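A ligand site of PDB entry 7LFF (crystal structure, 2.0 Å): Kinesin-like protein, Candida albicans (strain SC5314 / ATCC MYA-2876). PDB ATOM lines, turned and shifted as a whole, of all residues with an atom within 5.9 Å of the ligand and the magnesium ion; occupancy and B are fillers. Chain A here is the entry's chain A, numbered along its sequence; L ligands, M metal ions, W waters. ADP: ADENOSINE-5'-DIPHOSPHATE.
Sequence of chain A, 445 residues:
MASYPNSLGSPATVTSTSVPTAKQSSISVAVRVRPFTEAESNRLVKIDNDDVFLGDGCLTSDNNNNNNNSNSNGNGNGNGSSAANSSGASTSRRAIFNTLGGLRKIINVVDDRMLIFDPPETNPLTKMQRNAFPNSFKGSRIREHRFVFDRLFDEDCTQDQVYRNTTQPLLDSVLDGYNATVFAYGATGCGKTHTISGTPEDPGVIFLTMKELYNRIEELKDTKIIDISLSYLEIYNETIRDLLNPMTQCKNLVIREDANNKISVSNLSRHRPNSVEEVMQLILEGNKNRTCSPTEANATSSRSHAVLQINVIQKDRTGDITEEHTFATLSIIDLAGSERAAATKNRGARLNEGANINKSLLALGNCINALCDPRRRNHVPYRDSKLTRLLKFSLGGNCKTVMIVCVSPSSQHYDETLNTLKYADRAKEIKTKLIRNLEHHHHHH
Water W8 bridges an oxygen (O2') of the ligand and a ring nitrogen (ND1) of His 194. Water W2 bridges N6 of the ligand (2.7 Å) and NE of Arg 32 (3.1 Å). Water W9 lies within hydrogen-bond range of the backbone carbonyl oxygen (O) of Glu 155, the backbone carbonyl oxygen (O) of Cys 157 and a nitrogen (N6) of the ligand.
The guanidinium group of Arg 32 sits close to a nitrogen (N6) of the ligand, 3.2 Å away. Arg 34 touches the ligand (CB to N7, 3.99 Å). Pro 35 touches the ligand. O of Ala 187 touches O3B of the ligand (3.6 Å). Thr 188 touches the ligand (CG2 to O1B, 3.6 Å). Cys 190 touches the ligand (N to O3B, 3.5 Å). Hydrophobic or aromatic side chains within 4 Å of the ligand: Pro 35 and His 194. Within 4 Å of the ligand: Arg 32, Arg 34, Pro 35, Ala 187, Thr 188, Gly 189, Cys 190, Gly 191, Lys 192, Thr 193 and His 194. The nearest printed residue that does not touch the ligand is Asp 334 (4.6 Å).
The backbone carbonyl oxygen (O) of Gly 189 is in hydrogen-bond range of the guanidinium group (NE) of Arg 34, at 2.9 Å. The backbone carbonyl oxygen of Gly 186 lies within hydrogen-bond range of the side-chain amino group of Lys 192, 3.1 Å away. OG1 of Thr 193 lies close to OD2 of Asp 334 (2.6 Å). O of Ala 187 sits at hydrogen-bond distance from SG of Cys 190, at 3.3 Å. The guanidinium group of Arg 32 sits at hydrogen-bond distance from the side-chain hydroxyl of Thr 195 (2.8 Å). The guanidinium group of Arg 32 is in hydrogen-bond range of the side-chain amide oxygen of Gln 159. The side-chain sulfur (SG) of Cys 157 lies within hydrogen-bond range of the guanidinium group (NE) of Arg 32. O of Gly 191 sits at hydrogen-bond distance from OG1 of Thr 195 (2.6 Å).
Merely in contact with the magnesium ion: Asp 334. Two residues have an atom within 4 Å of the magnesium ion: Thr 193 and Asp 334.
The backbone NH (N) of Thr 193 sits at hydrogen-bond distance from an oxygen (O2A) of the ligand (3.1 Å). O3A of the ligand lies within hydrogen-bond range of N of Gly 191, 2.9 Å away. NE2 of His 194 sits close to N1 of the ligand, at 3.5 Å. The backbone NH (N) of His 194 lies within hydrogen-bond range of an oxygen (O2A) of the ligand, at 2.6 Å. The backbone NH (N) of Lys 192 is in hydrogen-bond range of an oxygen (O3B) of the ligand, at 2.8 Å. An oxygen (O3B) of the ligand lies within salt-bridge range of the side-chain amino group of Lys 192, 2.7 Å away. N of Gly 189 lies within hydrogen-bond range of O1B of the ligand (2.9 Å).
The magnesium ion is bound by water W7 (2.0 Å), water W5 (2.0 Å), OG1 of Thr 193 (2.0 Å), O2B of the ligand (2.2 Å), water W4 (2.2 Å) and water W3 (2.2 Å). The magnesium ion has six donor atoms within binding distance.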
ATOM      1  N   ARG A  32      -9.450  24.703  19.114  1.00  0.00           N
ATOM      2  CA  ARG A  32      -8.868  23.865  18.072  1.00  0.00           C
ATOM      3  C   ARG A  32      -9.727  22.620  17.904  1.00  0.00           C
ATOM      4  O   ARG A  32      -9.829  21.799  18.819  1.00  0.00           O
ATOM      5  CB  ARG A  32      -7.421  23.471  18.381  1.00  0.00           C
ATOM      6  CG  ARG A  32      -6.794  22.719  17.215  1.00  0.00           C
ATOM      7  CD  ARG A  32      -5.545  21.942  17.570  1.00  0.00           C
ATOM      8  NE  ARG A  32      -4.852  21.530  16.347  1.00  0.00           N
ATOM      9  CZ  ARG A  32      -3.599  21.077  16.298  1.00  0.00           C
ATOM     10  NH1 ARG A  32      -2.884  20.976  17.415  1.00  0.00           N
ATOM     11  NH2 ARG A  32      -3.070  20.735  15.142  1.00  0.00           N
ATOM     12  N   VAL A  33     -10.359  22.496  16.738  1.00  0.00           N
ATOM     13  CA  VAL A  33     -11.169  21.342  16.412  1.00  0.00           C
ATOM     14  C   VAL A  33     -10.248  20.275  15.833  1.00  0.00           C
ATOM     15  O   VAL A  33      -9.612  20.487  14.793  1.00  0.00           O
ATOM     16  CB  VAL A  33     -12.280  21.695  15.414  1.00  0.00           C
ATOM     17  CG1 VAL A  33     -13.295  20.571  15.314  1.00  0.00           C
ATOM     18  CG2 VAL A  33     -12.949  23.006  15.816  1.00  0.00           C
ATOM     19  N   ARG A  34     -10.166  19.127  16.504  1.00  0.00           N
ATOM     20  CA  ARG A  34      -9.391  18.024  15.957  1.00  0.00           C
ATOM     21  C   ARG A  34     -10.081  17.487  14.705  1.00  0.00           C
ATOM     22  O   ARG A  34     -11.294  17.618  14.554  1.00  0.00           O
ATOM     23  CB  ARG A  34      -9.224  16.918  16.996  1.00  0.00           C
ATOM     24  CG  ARG A  34     -10.386  15.932  17.073  1.00  0.00           C
ATOM     25  CD  ARG A  34      -9.911  14.560  17.559  1.00  0.00           C
ATOM     26  NE  ARG A  34     -10.998  13.721  18.030  1.00  0.00           N
ATOM     27  CZ  ARG A  34     -11.937  13.178  17.255  1.00  0.00           C
ATOM     28  NH1 ARG A  34     -11.919  13.384  15.942  1.00  0.00           N
ATOM     29  NH2 ARG A  34     -12.887  12.429  17.780  1.00  0.00           N
ATOM     30  N   PRO A  35      -9.328  16.912  13.776  1.00  0.00           N
ATOM     31  CA  PRO A  35      -9.954  16.328  12.583  1.00  0.00           C
ATOM     32  C   PRO A  35     -10.649  15.019  12.910  1.00  0.00           C
ATOM     33  O   PRO A  35     -10.431  14.405  13.962  1.00  0.00           O
ATOM     34  CB  PRO A  35      -8.773  16.106  11.633  1.00  0.00           C
ATOM     35  CG  PRO A  35      -7.580  16.006  12.524  1.00  0.00           C
ATOM     36  CD  PRO A  35      -7.859  16.915  13.686  1.00  0.00           C
ATOM     37  N   GLU A 155     -10.117  21.657  11.560  1.00  0.00           N
ATOM     38  CA  GLU A 155      -9.544  20.313  11.520  1.00  0.00           C
ATOM     39  C   GLU A 155      -8.220  20.245  10.777  1.00  0.00           C
ATOM     40  O   GLU A 155      -7.386  19.377  11.065  1.00  0.00           O
ATOM     41  CB  GLU A 155     -10.505  19.329  10.852  1.00  0.00           C
ATOM     42  CG  GLU A 155     -11.957  19.464  11.235  1.00  0.00           C
ATOM     43  CD  GLU A 155     -12.839  18.693  10.272  1.00  0.00           C
ATOM     44  OE1 GLU A 155     -12.628  17.478  10.118  1.00  0.00           O
ATOM     45  OE2 GLU A 155     -13.698  19.321   9.616  1.00  0.00           O
ATOM     46  N   CYS A 157      -5.881  22.762  10.396  1.00  0.00           N
ATOM     47  CA  CYS A 157      -4.838  23.709  10.778  1.00  0.00           C
ATOM     48  C   CYS A 157      -3.526  22.983  11.042  1.00  0.00           C
ATOM     49  O   CYS A 157      -3.501  21.800  11.389  1.00  0.00           O
ATOM     50  CB  CYS A 157      -5.258  24.489  12.027  1.00  0.00           C
ATOM     51  SG  CYS A 157      -5.224  23.497  13.544  1.00  0.00           S
ATOM     52  N   GLN A 159       0.370  22.603  12.920  1.00  0.00           N
ATOM     53  CA  GLN A 159       1.005  22.876  14.194  1.00  0.00           C
ATOM     54  C   GLN A 159       1.625  24.272  14.204  1.00  0.00           C
ATOM     55  O   GLN A 159       1.574  24.973  15.228  1.00  0.00           O
ATOM     56  CB  GLN A 159       2.083  21.824  14.491  1.00  0.00           C
ATOM     57  CG  GLN A 159       1.580  20.397  14.558  1.00  0.00           C
ATOM     58  CD  GLN A 159       0.841  20.075  15.850  1.00  0.00           C
ATOM     59  OE1 GLN A 159      -0.108  20.764  16.229  1.00  0.00           O
ATOM     60  NE2 GLN A 159       1.298  19.038  16.540  1.00  0.00           N
ATOM     61  N   GLY A 186      -9.655  20.257  27.447  1.00  0.00           N
ATOM     62  CA  GLY A 186     -10.634  19.565  26.642  1.00  0.00           C
ATOM     63  C   GLY A 186     -10.781  18.114  27.042  1.00  0.00           C
ATOM     64  O   GLY A 186     -10.036  17.587  27.875  1.00  0.00           O
ATOM     65  N   ALA A 187     -11.757  17.461  26.425  1.00  0.00           N
ATOM     66  CA  ALA A 187     -12.040  16.063  26.706  1.00  0.00           C
ATOM     67  C   ALA A 187     -10.963  15.162  26.135  1.00  0.00           C
ATOM     68  O   ALA A 187     -10.256  15.514  25.183  1.00  0.00           O
ATOM     69  CB  ALA A 187     -13.405  15.674  26.144  1.00  0.00           C
ATOM     70  N   THR A 188     -10.822  13.975  26.730  1.00  0.00           N
ATOM     71  CA  THR A 188      -9.855  13.000  26.262  1.00  0.00           C
ATOM     72  C   THR A 188     -10.141  12.625  24.811  1.00  0.00           C
ATOM     73  O   THR A 188     -11.297  12.391  24.433  1.00  0.00           O
ATOM     74  CB  THR A 188      -9.883  11.754  27.143  1.00  0.00           C
ATOM     75  OG1 THR A 188      -9.814  12.144  28.526  1.00  0.00           O
ATOM     76  CG2 THR A 188      -8.699  10.838  26.823  1.00  0.00           C
ATOM     77  N   GLY A 189      -9.084  12.567  24.000  1.00  0.00           N
ATOM     78  CA  GLY A 189      -9.199  12.233  22.605  1.00  0.00           C
ATOM     79  C   GLY A 189      -9.401  13.414  21.672  1.00  0.00           C
ATOM     80  O   GLY A 189      -9.598  13.194  20.467  1.00  0.00           O
ATOM     81  N   CYS A 190      -9.345  14.642  22.178  1.00  0.00           N
ATOM     82  CA  CYS A 190      -9.604  15.829  21.377  1.00  0.00           C
ATOM     83  C   CYS A 190      -8.332  16.545  20.945  1.00  0.00           C
ATOM     84  O   CYS A 190      -8.414  17.597  20.301  1.00  0.00           O
ATOM     85  CB  CYS A 190     -10.496  16.805  22.151  1.00  0.00           C
ATOM     86  SG  CYS A 190     -12.122  16.139  22.553  1.00  0.00           S
ATOM     87  N   GLY A 191      -7.152  15.999  21.254  1.00  0.00           N
ATOM     88  CA  GLY A 191      -5.916  16.539  20.744  1.00  0.00           C
ATOM     89  C   GLY A 191      -5.094  17.393  21.684  1.00  0.00           C
ATOM     90  O   GLY A 191      -4.280  18.180  21.206  1.00  0.00           O
ATOM     91  N   LYS A 192      -5.276  17.248  23.004  1.00  0.00           N
ATOM     92  CA  LYS A 192      -4.469  18.020  23.950  1.00  0.00           C
ATOM     93  C   LYS A 192      -2.992  17.671  23.814  1.00  0.00           C
ATOM     94  O   LYS A 192      -2.146  18.551  23.593  1.00  0.00           O
ATOM     95  CB  LYS A 192      -4.941  17.759  25.381  1.00  0.00           C
ATOM     96  CG  LYS A 192      -6.279  18.395  25.733  1.00  0.00           C
ATOM     97  CD  LYS A 192      -6.614  18.202  27.212  1.00  0.00           C
ATOM     98  CE  LYS A 192      -6.553  16.739  27.629  1.00  0.00           C
ATOM     99  NZ  LYS A 192      -7.577  15.908  26.937  1.00  0.00           N
ATOM    100  N   THR A 193      -2.667  16.385  23.941  1.00  0.00           N
ATOM    101  CA  THR A 193      -1.269  15.947  23.854  1.00  0.00           C
ATOM    102  C   THR A 193      -0.696  16.192  22.470  1.00  0.00           C
ATOM    103  O   THR A 193       0.484  16.541  22.331  1.00  0.00           O
ATOM    104  CB  THR A 193      -1.162  14.473  24.245  1.00  0.00           C
ATOM    105  OG1 THR A 193      -1.676  14.295  25.577  1.00  0.00           O
ATOM    106  CG2 THR A 193       0.287  14.005  24.206  1.00  0.00           C
ATOM    107  N   HIS A 194      -1.516  16.003  21.430  1.00  0.00           N
ATOM    108  CA  HIS A 194      -1.063  16.293  20.069  1.00  0.00           C
ATOM    109  C   HIS A 194      -0.698  17.769  19.925  1.00  0.00           C
ATOM    110  O   HIS A 194       0.271  18.109  19.238  1.00  0.00           O
ATOM    111  CB  HIS A 194      -2.142  15.908  19.065  1.00  0.00           C
ATOM    112  CG  HIS A 194      -1.782  16.213  17.646  1.00  0.00           C
ATOM    113  ND1 HIS A 194      -0.881  15.459  16.926  1.00  0.00           N
ATOM    114  CD2 HIS A 194      -2.170  17.204  16.818  1.00  0.00           C
ATOM    115  CE1 HIS A 194      -0.745  15.963  15.719  1.00  0.00           C
ATOM    116  NE2 HIS A 194      -1.523  17.027  15.625  1.00  0.00           N
ATOM    117  N   THR A 195      -1.457  18.654  20.567  1.00  0.00           N
ATOM    118  CA  THR A 195      -1.187  20.085  20.447  1.00  0.00           C
ATOM    119  C   THR A 195       0.040  20.483  21.259  1.00  0.00           C
ATOM    120  O   THR A 195       0.883  21.250  20.769  1.00  0.00           O
ATOM    121  CB  THR A 195      -2.413  20.876  20.898  1.00  0.00           C
ATOM    122  OG1 THR A 195      -3.550  20.473  20.133  1.00  0.00           O
ATOM    123  CG2 THR A 195      -2.172  22.375  20.699  1.00  0.00           C
ATOM    124  N   THR A 199       4.058  14.833  17.698  1.00  0.00           N
ATOM    125  CA  THR A 199       4.824  13.663  17.308  1.00  0.00           C
ATOM    126  C   THR A 199       6.166  14.089  16.737  1.00  0.00           C
ATOM    127  O   THR A 199       6.344  15.266  16.387  1.00  0.00           O
ATOM    128  CB  THR A 199       4.042  12.836  16.264  1.00  0.00           C
ATOM    129  OG1 THR A 199       3.768  13.644  15.118  1.00  0.00           O
ATOM    130  CG2 THR A 199       2.727  12.333  16.853  1.00  0.00           C
ATOM    131  N   ASP A 202       5.318  15.534  13.476  1.00  0.00           N
ATOM    132  CA  ASP A 202       4.468  16.726  13.517  1.00  0.00           C
ATOM    133  C   ASP A 202       4.558  17.331  14.903  1.00  0.00           C
ATOM    134  O   ASP A 202       3.634  17.207  15.721  1.00  0.00           O
ATOM    135  CB  ASP A 202       3.033  16.381  13.144  1.00  0.00           C
ATOM    136  CG  ASP A 202       2.261  17.571  12.607  1.00  0.00           C
ATOM    137  OD1 ASP A 202       2.899  18.562  12.219  1.00  0.00           O
ATOM    138  OD2 ASP A 202       1.009  17.507  12.587  1.00  0.00           O
ATOM    139  N   ARG A 290       4.313   9.139  32.207  1.00  0.00           N
ATOM    140  CA  ARG A 290       3.074   9.582  32.841  1.00  0.00           C
ATOM    141  C   ARG A 290       2.280   8.389  33.382  1.00  0.00           C
ATOM    142  O   ARG A 290       2.409   7.261  32.910  1.00  0.00           O
ATOM    143  CB  ARG A 290       2.222  10.374  31.869  1.00  0.00           C
ATOM    144  CG  ARG A 290       2.646  11.821  31.710  1.00  0.00           C
ATOM    145  CD  ARG A 290       2.075  12.448  30.450  1.00  0.00           C
ATOM    146  NE  ARG A 290       0.788  13.102  30.697  1.00  0.00           N
ATOM    147  CZ  ARG A 290       0.232  13.978  29.866  1.00  0.00           C
ATOM    148  NH1 ARG A 290       0.848  14.318  28.746  1.00  0.00           N
ATOM    149  NH2 ARG A 290      -0.937  14.518  30.174  1.00  0.00           N
ATOM    150  N   THR A 300      -1.898   6.731  28.807  1.00  0.00           N
ATOM    151  CA  THR A 300      -1.810   7.758  29.835  1.00  0.00           C
ATOM    152  C   THR A 300      -3.183   7.976  30.458  1.00  0.00           C
ATOM    153  O   THR A 300      -4.175   8.148  29.737  1.00  0.00           O
ATOM    154  CB  THR A 300      -1.287   9.062  29.229  1.00  0.00           C
ATOM    155  OG1 THR A 300       0.027   8.862  28.685  1.00  0.00           O
ATOM    156  CG2 THR A 300      -1.226  10.153  30.292  1.00  0.00           C
ATOM    157  N   ASP A 334      -0.282  20.376  29.364  1.00  0.00           N
ATOM    158  CA  ASP A 334      -1.223  19.399  28.805  1.00  0.00           C
ATOM    159  C   ASP A 334      -2.079  18.938  29.976  1.00  0.00           C
ATOM    160  O   ASP A 334      -1.650  18.132  30.797  1.00  0.00           O
ATOM    161  CB  ASP A 334      -0.457  18.258  28.142  1.00  0.00           C
ATOM    162  CG  ASP A 334      -1.360  17.176  27.604  1.00  0.00           C
ATOM    163  OD1 ASP A 334      -2.591  17.358  27.592  1.00  0.00           O
ATOM    164  OD2 ASP A 334      -0.819  16.126  27.181  1.00  0.00           O
ATOM    165  N   LEU A 335      -3.286  19.495  30.082  1.00  0.00           N
ATOM    166  CA  LEU A 335      -4.113  19.279  31.248  1.00  0.00           C
ATOM    167  C   LEU A 335      -4.730  17.886  31.257  1.00  0.00           C
ATOM    168  O   LEU A 335      -4.770  17.189  30.239  1.00  0.00           O
ATOM    169  CB  LEU A 335      -5.226  20.324  31.318  1.00  0.00           C
ATOM    170  CG  LEU A 335      -4.845  21.763  31.651  1.00  0.00           C
ATOM    171  CD1 LEU A 335      -6.016  22.689  31.370  1.00  0.00           C
ATOM    172  CD2 LEU A 335      -4.424  21.864  33.103  1.00  0.00           C
ATOM    173  N   CYS A 406      -9.721  22.300  23.149  1.00  0.00           N
ATOM    174  CA  CYS A 406      -9.653  21.257  22.138  1.00  0.00           C
ATOM    175  C   CYS A 406     -10.959  20.483  22.144  1.00  0.00           C
ATOM    176  O   CYS A 406     -11.326  19.884  23.171  1.00  0.00           O
ATOM    177  CB  CYS A 406      -8.475  20.328  22.398  1.00  0.00           C
ATOM    178  SG  CYS A 406      -6.848  21.134  22.373  1.00  0.00           S
HETATM  179  PB  ADP L   1      -5.840  14.083  24.266  1.00  0.00           P
HETATM  180  O1B ADP L   1      -6.379  12.834  24.907  1.00  0.00           O
HETATM  181  O2B ADP L   1      -4.375  14.336  24.557  1.00  0.00           O
HETATM  182  O3B ADP L   1      -6.721  15.300  24.422  1.00  0.00           O
HETATM  183  PA  ADP L   1      -4.579  13.332  21.879  1.00  0.00           P
HETATM  184  O1A ADP L   1      -4.020  12.081  22.515  1.00  0.00           O
HETATM  185  O2A ADP L   1      -3.696  14.549  21.720  1.00  0.00           O
HETATM  186  O3A ADP L   1      -5.896  13.766  22.693  1.00  0.00           O
HETATM  187  O5' ADP L   1      -5.158  12.935  20.431  1.00  0.00           O
HETATM  188  C5' ADP L   1      -6.022  11.811  20.264  1.00  0.00           C
HETATM  189  C4' ADP L   1      -5.639  11.141  18.951  1.00  0.00           C
HETATM  190  O4' ADP L   1      -6.026  11.970  17.862  1.00  0.00           O
HETATM  191  C3' ADP L   1      -4.130  10.954  18.865  1.00  0.00           C
HETATM  192  O3' ADP L   1      -3.836   9.663  18.309  1.00  0.00           O
HETATM  193  C2' ADP L   1      -3.662  12.026  17.896  1.00  0.00           C
HETATM  194  O2' ADP L   1      -2.597  11.543  17.083  1.00  0.00           O
HETATM  195  C1' ADP L   1      -4.892  12.348  17.079  1.00  0.00           C
HETATM  196  N9  ADP L   1      -4.980  13.799  16.791  1.00  0.00           N
HETATM  197  C8  ADP L   1      -5.394  14.734  17.663  1.00  0.00           C
HETATM  198  N7  ADP L   1      -5.348  15.970  17.100  1.00  0.00           N
HETATM  199  C5  ADP L   1      -4.899  15.818  15.834  1.00  0.00           C
HETATM  200  C6  ADP L   1      -4.617  16.718  14.690  1.00  0.00           C
HETATM  201  N6  ADP L   1      -4.813  18.058  14.789  1.00  0.00           N
HETATM  202  N1  ADP L   1      -4.157  16.161  13.551  1.00  0.00           N
HETATM  203  C2  ADP L   1      -3.962  14.831  13.450  1.00  0.00           C
HETATM  204  N3  ADP L   1      -4.190  13.963  14.447  1.00  0.00           N
HETATM  205  C4  ADP L   1      -4.655  14.386  15.639  1.00  0.00           C
HETATM  206 MG    MG M   1      -3.384  13.402  26.258  1.00  0.00          MG
HETATM  207  O   HOH W   1      -6.216  10.418  23.964  1.00  0.00           O
HETATM  208  O   HOH W   2      -5.533  18.680  17.268  1.00  0.00           O
HETATM  209  O   HOH W   3      -5.005  12.116  27.040  1.00  0.00           O
HETATM  210  O   HOH W   4      -2.907  11.744  24.878  1.00  0.00           O
HETATM  211  O   HOH W   5      -3.851  14.961  27.447  1.00  0.00           O
HETATM  212  O   HOH W   6      -8.574  11.239  17.026  1.00  0.00           O
HETATM  213  O   HOH W   7      -2.181  12.195  27.269  1.00  0.00           O
HETATM  214  O   HOH W   8      -0.485  12.595  17.776  1.00  0.00           O
HETATM  215  O   HOH W   9      -5.049  19.759  12.109  1.00  0.00           O
